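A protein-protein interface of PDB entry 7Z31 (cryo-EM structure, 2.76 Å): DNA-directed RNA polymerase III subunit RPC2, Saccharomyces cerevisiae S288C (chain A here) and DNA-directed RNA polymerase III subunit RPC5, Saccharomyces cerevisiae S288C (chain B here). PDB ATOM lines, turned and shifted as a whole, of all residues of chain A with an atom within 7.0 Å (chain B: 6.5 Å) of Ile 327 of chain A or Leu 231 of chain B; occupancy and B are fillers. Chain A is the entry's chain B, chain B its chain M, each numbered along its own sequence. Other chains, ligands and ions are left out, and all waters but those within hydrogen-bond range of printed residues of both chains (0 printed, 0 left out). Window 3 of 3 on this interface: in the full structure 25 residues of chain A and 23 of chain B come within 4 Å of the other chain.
A ring nitrogen (NE2) of His 234 of chain B lies within hydrogen-bond range of the side-chain hydroxyl of Ser 230 of chain B, at 3.4 Å. OG1 of Thr 330 of chain A sits at hydrogen-bond distance from O of Ala 326 of chain A, 2.7 Å away.
Of the 10 printed residues of chain B, 4 touch a printed residue of chain A. Of the 19 printed residues of chain A, 6 touch a printed residue of chain B. Printed residues of chain A that touch a printed residue of chain B: Gly 323, Ala 326, Ile 327, Val 337, Glu 338 and Ala 339. Hydrophobic or aromatic side chains of chain A within 4 Å of the printed part of chain B: Ala 326 and Ile 327. Among the printed residues, 7 pairs touch across the chains.
Met 312 of chain A touches none of the printed residues of chain B. Of the printed residues of chain B, Gly 323 of chain A touches Leu 231. Of the printed residues of chain B, Ala 326 of chain A touches Leu 231 (3.5 Å). Of chain B, only Leu 231 (3.8 Å) comes within 4 Å of Ile 327 of chain A. Of the printed residues of chain B, Ala 339 of chain A touches Ser 230 (2.9 Å) and Ala 233 (3.96 Å). Of the printed residues of chain A, Gly 229 of chain B touches Glu 338. Of the printed residues of chain A, Leu 231 of chain B touches Gly 323, Ala 326 and Ile 327. The nearest residue of chain B that does not touch Ile 327 of chain A is Thr 228 of chain B (6.3 Å).
The side-chain hydroxyl (OG) of Ser 230 of chain B is in hydrogen-bond range of the backbone carbonyl oxygen (O) of Ala 339 of chain A (2.9 Å).
Leu 231 of chain B touches Gly 323 of chain A (CD2 to O, 3.2 Å). Ala 326 of chain A touches Leu 231 of chain B (CB to CD2, 3.5 Å). CG2 of Ile 327 of chain A touches CD2 of Leu 231 of chain B, 3.8 Å away. O of Val 337 of chain A touches CB of Ser 230 of chain B, 3.6 Å away. Gly 229 of chain B touches Glu 338 of chain A (CA to OE2, 3.8 Å). Ala 233 of chain B touches Ala 339 of chain A.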
ATOM      1  N   ARG A 227      17.833  40.334   0.965  1.00  0.00           N
ATOM      2  CA  ARG A 227      18.518  40.325  -0.320  1.00  0.00           C
ATOM      3  C   ARG A 227      17.517  40.416  -1.461  1.00  0.00           C
ATOM      4  O   ARG A 227      16.366  39.990  -1.339  1.00  0.00           O
ATOM      5  CB  ARG A 227      19.371  39.065  -0.493  1.00  0.00           C
ATOM      6  CG  ARG A 227      20.564  39.005   0.423  1.00  0.00           C
ATOM      7  CD  ARG A 227      21.377  37.751   0.188  1.00  0.00           C
ATOM      8  NE  ARG A 227      22.635  37.797   0.923  1.00  0.00           N
ATOM      9  CZ  ARG A 227      23.341  36.731   1.267  1.00  0.00           C
ATOM     10  NH1 ARG A 227      22.928  35.508   0.980  1.00  0.00           N
ATOM     11  NH2 ARG A 227      24.485  36.896   1.924  1.00  0.00           N
ATOM     12  N   SER A 246      25.706  36.674  -8.533  1.00  0.00           N
ATOM     13  CA  SER A 246      26.764  36.188  -7.658  1.00  0.00           C
ATOM     14  C   SER A 246      27.691  35.229  -8.388  1.00  0.00           C
ATOM     15  O   SER A 246      28.915  35.338  -8.278  1.00  0.00           O
ATOM     16  CB  SER A 246      26.162  35.503  -6.434  1.00  0.00           C
ATOM     17  OG  SER A 246      25.948  34.126  -6.685  1.00  0.00           O
ATOM     18  N   VAL A 309      31.512  30.705  -7.282  1.00  0.00           N
ATOM     19  CA  VAL A 309      30.899  31.706  -6.420  1.00  0.00           C
ATOM     20  C   VAL A 309      31.962  32.731  -6.056  1.00  0.00           C
ATOM     21  O   VAL A 309      32.972  32.394  -5.426  1.00  0.00           O
ATOM     22  CB  VAL A 309      30.291  31.046  -5.185  1.00  0.00           C
ATOM     23  CG1 VAL A 309      29.189  31.911  -4.611  1.00  0.00           C
ATOM     24  CG2 VAL A 309      29.770  29.662  -5.540  1.00  0.00           C
ATOM     25  N   MET A 312      32.894  36.794  -0.714  1.00  0.00           N
ATOM     26  CA  MET A 312      32.047  37.361   0.331  1.00  0.00           C
ATOM     27  C   MET A 312      32.811  38.422   1.114  1.00  0.00           C
ATOM     28  O   MET A 312      32.795  38.440   2.350  1.00  0.00           O
ATOM     29  CB  MET A 312      31.518  36.269   1.261  1.00  0.00           C
ATOM     30  CG  MET A 312      32.588  35.297   1.722  1.00  0.00           C
ATOM     31  SD  MET A 312      31.958  33.801   2.493  1.00  0.00           S
ATOM     32  CE  MET A 312      33.485  32.889   2.671  1.00  0.00           C
ATOM     33  N   LYS A 316      34.878  34.966   6.820  1.00  0.00           N
ATOM     34  CA  LYS A 316      34.635  33.528   6.940  1.00  0.00           C
ATOM     35  C   LYS A 316      35.383  32.760   5.849  1.00  0.00           C
ATOM     36  O   LYS A 316      34.866  31.810   5.260  1.00  0.00           O
ATOM     37  CB  LYS A 316      33.133  33.218   6.914  1.00  0.00           C
ATOM     38  CG  LYS A 316      32.750  31.823   7.397  1.00  0.00           C
ATOM     39  CD  LYS A 316      33.578  31.429   8.607  1.00  0.00           C
ATOM     40  CE  LYS A 316      33.523  29.932   8.849  1.00  0.00           C
ATOM     41  NZ  LYS A 316      32.166  29.477   9.249  1.00  0.00           N
ATOM     42  N   ILE A 319      35.648  28.761   4.553  1.00  0.00           N
ATOM     43  CA  ILE A 319      34.538  27.977   4.022  1.00  0.00           C
ATOM     44  C   ILE A 319      34.673  27.703   2.532  1.00  0.00           C
ATOM     45  O   ILE A 319      33.811  27.016   1.959  1.00  0.00           O
ATOM     46  CB  ILE A 319      33.186  28.649   4.334  1.00  0.00           C
ATOM     47  CG1 ILE A 319      32.125  27.594   4.670  1.00  0.00           C
ATOM     48  CG2 ILE A 319      32.734  29.549   3.191  1.00  0.00           C
ATOM     49  CD1 ILE A 319      30.788  28.179   5.083  1.00  0.00           C
ATOM     50  N   GLY A 323      31.544  23.256   0.793  1.00  0.00           N
ATOM     51  CA  GLY A 323      30.609  23.893   1.697  1.00  0.00           C
ATOM     52  C   GLY A 323      30.181  25.289   1.314  1.00  0.00           C
ATOM     53  O   GLY A 323      29.423  25.921   2.055  1.00  0.00           O
ATOM     54  N   ILE A 324      30.660  25.807   0.181  1.00  0.00           N
ATOM     55  CA  ILE A 324      30.179  27.090  -0.317  1.00  0.00           C
ATOM     56  C   ILE A 324      28.976  26.911  -1.235  1.00  0.00           C
ATOM     57  O   ILE A 324      28.178  27.849  -1.398  1.00  0.00           O
ATOM     58  CB  ILE A 324      31.318  27.839  -1.030  1.00  0.00           C
ATOM     59  CG1 ILE A 324      31.035  29.339  -1.095  1.00  0.00           C
ATOM     60  CG2 ILE A 324      31.534  27.295  -2.418  1.00  0.00           C
ATOM     61  CD1 ILE A 324      32.203  30.141  -1.602  1.00  0.00           C
ATOM     62  N   GLU A 325      28.810  25.715  -1.814  1.00  0.00           N
ATOM     63  CA  GLU A 325      27.662  25.452  -2.671  1.00  0.00           C
ATOM     64  C   GLU A 325      26.355  25.660  -1.934  1.00  0.00           C
ATOM     65  O   GLU A 325      25.335  25.943  -2.561  1.00  0.00           O
ATOM     66  CB  GLU A 325      27.705  24.022  -3.221  1.00  0.00           C
ATOM     67  CG  GLU A 325      27.498  22.897  -2.181  1.00  0.00           C
ATOM     68  CD  GLU A 325      26.078  22.770  -1.633  1.00  0.00           C
ATOM     69  OE1 GLU A 325      25.116  23.068  -2.373  1.00  0.00           O
ATOM     70  OE2 GLU A 325      25.930  22.405  -0.446  1.00  0.00           O
ATOM     71  N   ALA A 326      26.347  25.461  -0.616  1.00  0.00           N
ATOM     72  CA  ALA A 326      25.090  25.542   0.112  1.00  0.00           C
ATOM     73  C   ALA A 326      24.527  26.951   0.048  1.00  0.00           C
ATOM     74  O   ALA A 326      23.352  27.145  -0.272  1.00  0.00           O
ATOM     75  CB  ALA A 326      25.282  25.089   1.556  1.00  0.00           C
ATOM     76  N   ILE A 327      25.360  27.954   0.324  1.00  0.00           N
ATOM     77  CA  ILE A 327      24.871  29.320   0.219  1.00  0.00           C
ATOM     78  C   ILE A 327      24.819  29.755  -1.239  1.00  0.00           C
ATOM     79  O   ILE A 327      24.073  30.678  -1.586  1.00  0.00           O
ATOM     80  CB  ILE A 327      25.716  30.270   1.087  1.00  0.00           C
ATOM     81  CG1 ILE A 327      27.201  30.147   0.759  1.00  0.00           C
ATOM     82  CG2 ILE A 327      25.474  29.984   2.564  1.00  0.00           C
ATOM     83  CD1 ILE A 327      28.089  30.991   1.669  1.00  0.00           C
ATOM     84  N   ALA A 328      25.569  29.089  -2.122  1.00  0.00           N
ATOM     85  CA  ALA A 328      25.394  29.339  -3.550  1.00  0.00           C
ATOM     86  C   ALA A 328      23.990  28.962  -4.009  1.00  0.00           C
ATOM     87  O   ALA A 328      23.376  29.675  -4.810  1.00  0.00           O
ATOM     88  CB  ALA A 328      26.435  28.565  -4.356  1.00  0.00           C
ATOM     89  N   THR A 329      23.465  27.846  -3.504  1.00  0.00           N
ATOM     90  CA  THR A 329      22.154  27.362  -3.924  1.00  0.00           C
ATOM     91  C   THR A 329      21.032  28.017  -3.126  1.00  0.00           C
ATOM     92  O   THR A 329      19.950  28.269  -3.666  1.00  0.00           O
ATOM     93  CB  THR A 329      22.106  25.836  -3.813  1.00  0.00           C
ATOM     94  OG1 THR A 329      22.538  25.257  -5.050  1.00  0.00           O
ATOM     95  CG2 THR A 329      20.711  25.340  -3.490  1.00  0.00           C
ATOM     96  N   THR A 330      21.278  28.338  -1.855  1.00  0.00           N
ATOM     97  CA  THR A 330      20.289  29.061  -1.067  1.00  0.00           C
ATOM     98  C   THR A 330      20.328  30.564  -1.335  1.00  0.00           C
ATOM     99  O   THR A 330      19.495  31.305  -0.802  1.00  0.00           O
ATOM    100  CB  THR A 330      20.498  28.756   0.414  1.00  0.00           C
ATOM    101  OG1 THR A 330      20.768  27.357   0.562  1.00  0.00           O
ATOM    102  CG2 THR A 330      19.250  29.092   1.214  1.00  0.00           C
ATOM    103  N   VAL A 331      21.276  31.035  -2.147  1.00  0.00           N
ATOM    104  CA  VAL A 331      21.228  32.390  -2.671  1.00  0.00           C
ATOM    105  C   VAL A 331      20.753  32.425  -4.114  1.00  0.00           C
ATOM    106  O   VAL A 331      20.559  33.513  -4.672  1.00  0.00           O
ATOM    107  CB  VAL A 331      22.599  33.082  -2.537  1.00  0.00           C
ATOM    108  CG1 VAL A 331      23.423  32.912  -3.809  1.00  0.00           C
ATOM    109  CG2 VAL A 331      22.413  34.552  -2.177  1.00  0.00           C
ATOM    110  N   ILE A 332      20.527  31.261  -4.726  1.00  0.00           N
ATOM    111  CA  ILE A 332      20.174  31.208  -6.137  1.00  0.00           C
ATOM    112  C   ILE A 332      18.739  31.651  -6.391  1.00  0.00           C
ATOM    113  O   ILE A 332      18.372  31.899  -7.543  1.00  0.00           O
ATOM    114  CB  ILE A 332      20.408  29.789  -6.685  1.00  0.00           C
ATOM    115  CG1 ILE A 332      20.943  29.861  -8.108  1.00  0.00           C
ATOM    116  CG2 ILE A 332      19.126  28.969  -6.633  1.00  0.00           C
ATOM    117  CD1 ILE A 332      22.369  30.350  -8.183  1.00  0.00           C
ATOM    118  N   VAL A 337      16.262  26.937   1.293  1.00  0.00           N
ATOM    119  CA  VAL A 337      16.364  25.531   1.666  1.00  0.00           C
ATOM    120  C   VAL A 337      17.319  25.421   2.846  1.00  0.00           C
ATOM    121  O   VAL A 337      18.474  25.853   2.764  1.00  0.00           O
ATOM    122  CB  VAL A 337      16.834  24.665   0.487  1.00  0.00           C
ATOM    123  CG1 VAL A 337      17.922  25.371  -0.308  1.00  0.00           C
ATOM    124  CG2 VAL A 337      17.333  23.329   0.993  1.00  0.00           C
ATOM    125  N   GLU A 338      16.839  24.850   3.946  1.00  0.00           N
ATOM    126  CA  GLU A 338      17.585  24.778   5.195  1.00  0.00           C
ATOM    127  C   GLU A 338      17.720  23.342   5.692  1.00  0.00           C
ATOM    128  O   GLU A 338      17.670  23.081   6.895  1.00  0.00           O
ATOM    129  CB  GLU A 338      16.928  25.637   6.272  1.00  0.00           C
ATOM    130  CG  GLU A 338      17.265  27.113   6.218  1.00  0.00           C
ATOM    131  CD  GLU A 338      17.150  27.773   7.585  1.00  0.00           C
ATOM    132  OE1 GLU A 338      16.393  27.254   8.430  1.00  0.00           O
ATOM    133  OE2 GLU A 338      17.822  28.800   7.816  1.00  0.00           O
ATOM    134  N   ALA A 339      17.901  22.391   4.785  1.00  0.00           N
ATOM    135  CA  ALA A 339      17.942  20.991   5.182  1.00  0.00           C
ATOM    136  C   ALA A 339      18.646  20.189   4.093  1.00  0.00           C
ATOM    137  O   ALA A 339      19.318  20.745   3.219  1.00  0.00           O
ATOM    138  CB  ALA A 339      16.533  20.464   5.462  1.00  0.00           C
ATOM    139  N   LEU B 227      27.726  28.557  11.337  1.00  0.00           N
ATOM    140  CA  LEU B 227      27.356  27.482  10.415  1.00  0.00           C
ATOM    141  C   LEU B 227      25.861  27.155  10.528  1.00  0.00           C
ATOM    142  O   LEU B 227      25.448  26.100  11.007  1.00  0.00           O
ATOM    143  CB  LEU B 227      28.223  26.241  10.658  1.00  0.00           C
ATOM    144  CG  LEU B 227      28.000  25.018   9.774  1.00  0.00           C
ATOM    145  CD1 LEU B 227      28.937  25.022   8.577  1.00  0.00           C
ATOM    146  CD2 LEU B 227      28.177  23.775  10.623  1.00  0.00           C
ATOM    147  N   THR B 228      25.059  28.128  10.112  1.00  0.00           N
ATOM    148  CA  THR B 228      23.610  28.026  10.159  1.00  0.00           C
ATOM    149  C   THR B 228      23.078  27.487   8.831  1.00  0.00           C
ATOM    150  O   THR B 228      23.839  27.124   7.932  1.00  0.00           O
ATOM    151  CB  THR B 228      23.006  29.389  10.495  1.00  0.00           C
ATOM    152  OG1 THR B 228      21.578  29.288  10.534  1.00  0.00           O
ATOM    153  CG2 THR B 228      23.415  30.422   9.451  1.00  0.00           C
ATOM    154  N   GLY B 229      21.753  27.431   8.701  1.00  0.00           N
ATOM    155  CA  GLY B 229      21.121  27.046   7.454  1.00  0.00           C
ATOM    156  C   GLY B 229      21.427  25.616   7.042  1.00  0.00           C
ATOM    157  O   GLY B 229      21.532  24.704   7.864  1.00  0.00           O
ATOM    158  N   SER B 230      21.560  25.422   5.728  1.00  0.00           N
ATOM    159  CA  SER B 230      21.862  24.106   5.177  1.00  0.00           C
ATOM    160  C   SER B 230      23.345  23.771   5.242  1.00  0.00           C
ATOM    161  O   SER B 230      23.708  22.612   5.019  1.00  0.00           O
ATOM    162  CB  SER B 230      21.369  24.017   3.731  1.00  0.00           C
ATOM    163  OG  SER B 230      21.501  22.701   3.228  1.00  0.00           O
ATOM    164  N   LEU B 231      24.206  24.752   5.523  1.00  0.00           N
ATOM    165  CA  LEU B 231      25.598  24.437   5.817  1.00  0.00           C
ATOM    166  C   LEU B 231      25.683  23.481   6.997  1.00  0.00           C
ATOM    167  O   LEU B 231      26.387  22.464   6.940  1.00  0.00           O
ATOM    168  CB  LEU B 231      26.374  25.717   6.120  1.00  0.00           C
ATOM    169  CG  LEU B 231      26.127  26.932   5.231  1.00  0.00           C
ATOM    170  CD1 LEU B 231      26.324  28.224   6.012  1.00  0.00           C
ATOM    171  CD2 LEU B 231      27.046  26.894   4.034  1.00  0.00           C
ATOM    172  N   LEU B 232      24.945  23.787   8.066  1.00  0.00           N
ATOM    173  CA  LEU B 232      24.887  22.906   9.223  1.00  0.00           C
ATOM    174  C   LEU B 232      24.376  21.525   8.849  1.00  0.00           C
ATOM    175  O   LEU B 232      24.804  20.536   9.442  1.00  0.00           O
ATOM    176  CB  LEU B 232      24.005  23.529  10.304  1.00  0.00           C
ATOM    177  CG  LEU B 232      23.725  22.789  11.614  1.00  0.00           C
ATOM    178  CD1 LEU B 232      25.010  22.385  12.329  1.00  0.00           C
ATOM    179  CD2 LEU B 232      22.865  23.658  12.511  1.00  0.00           C
ATOM    180  N   ALA B 233      23.495  21.429   7.852  1.00  0.00           N
ATOM    181  CA  ALA B 233      22.937  20.130   7.487  1.00  0.00           C
ATOM    182  C   ALA B 233      24.016  19.192   6.957  1.00  0.00           C
ATOM    183  O   ALA B 233      24.161  18.061   7.430  1.00  0.00           O
ATOM    184  CB  ALA B 233      21.825  20.307   6.455  1.00  0.00           C
ATOM    185  N   HIS B 234      24.805  19.653   5.986  1.00  0.00           N
ATOM    186  CA  HIS B 234      25.827  18.787   5.415  1.00  0.00           C
ATOM    187  C   HIS B 234      27.034  18.655   6.336  1.00  0.00           C
ATOM    188  O   HIS B 234      27.713  17.619   6.322  1.00  0.00           O
ATOM    189  CB  HIS B 234      26.228  19.303   4.035  1.00  0.00           C
ATOM    190  CG  HIS B 234      25.070  19.446   3.097  1.00  0.00           C
ATOM    191  ND1 HIS B 234      24.791  18.521   2.115  1.00  0.00           N
ATOM    192  CD2 HIS B 234      24.107  20.392   3.007  1.00  0.00           C
ATOM    193  CE1 HIS B 234      23.712  18.897   1.452  1.00  0.00           C
ATOM    194  NE2 HIS B 234      23.277  20.030   1.973  1.00  0.00           N
ATOM    195  N   LYS B 235      27.308  19.673   7.155  1.00  0.00           N
ATOM    196  CA  LYS B 235      28.349  19.528   8.164  1.00  0.00           C
ATOM    197  C   LYS B 235      27.965  18.466   9.189  1.00  0.00           C
ATOM    198  O   LYS B 235      28.797  17.649   9.591  1.00  0.00           O
ATOM    199  CB  LYS B 235      28.619  20.870   8.837  1.00  0.00           C
ATOM    200  CG  LYS B 235      30.071  21.106   9.229  1.00  0.00           C
ATOM    201  CD  LYS B 235      30.944  21.367   8.014  1.00  0.00           C
ATOM    202  CE  LYS B 235      32.339  21.809   8.421  1.00  0.00           C
ATOM    203  NZ  LYS B 235      32.714  23.089   7.761  1.00  0.00           N
ATOM    204  N   VAL B 236      26.698  18.446   9.604  1.00  0.00           N
ATOM    205  CA  VAL B 236      26.201  17.368  10.449  1.00  0.00           C
ATOM    206  C   VAL B 236      26.307  16.039   9.719  1.00  0.00           C
ATOM    207  O   VAL B 236      26.743  15.038  10.294  1.00  0.00           O
ATOM    208  CB  VAL B 236      24.755  17.665  10.886  1.00  0.00           C
ATOM    209  CG1 VAL B 236      24.045  16.382  11.307  1.00  0.00           C
ATOM    210  CG2 VAL B 236      24.750  18.679  12.015  1.00  0.00           C
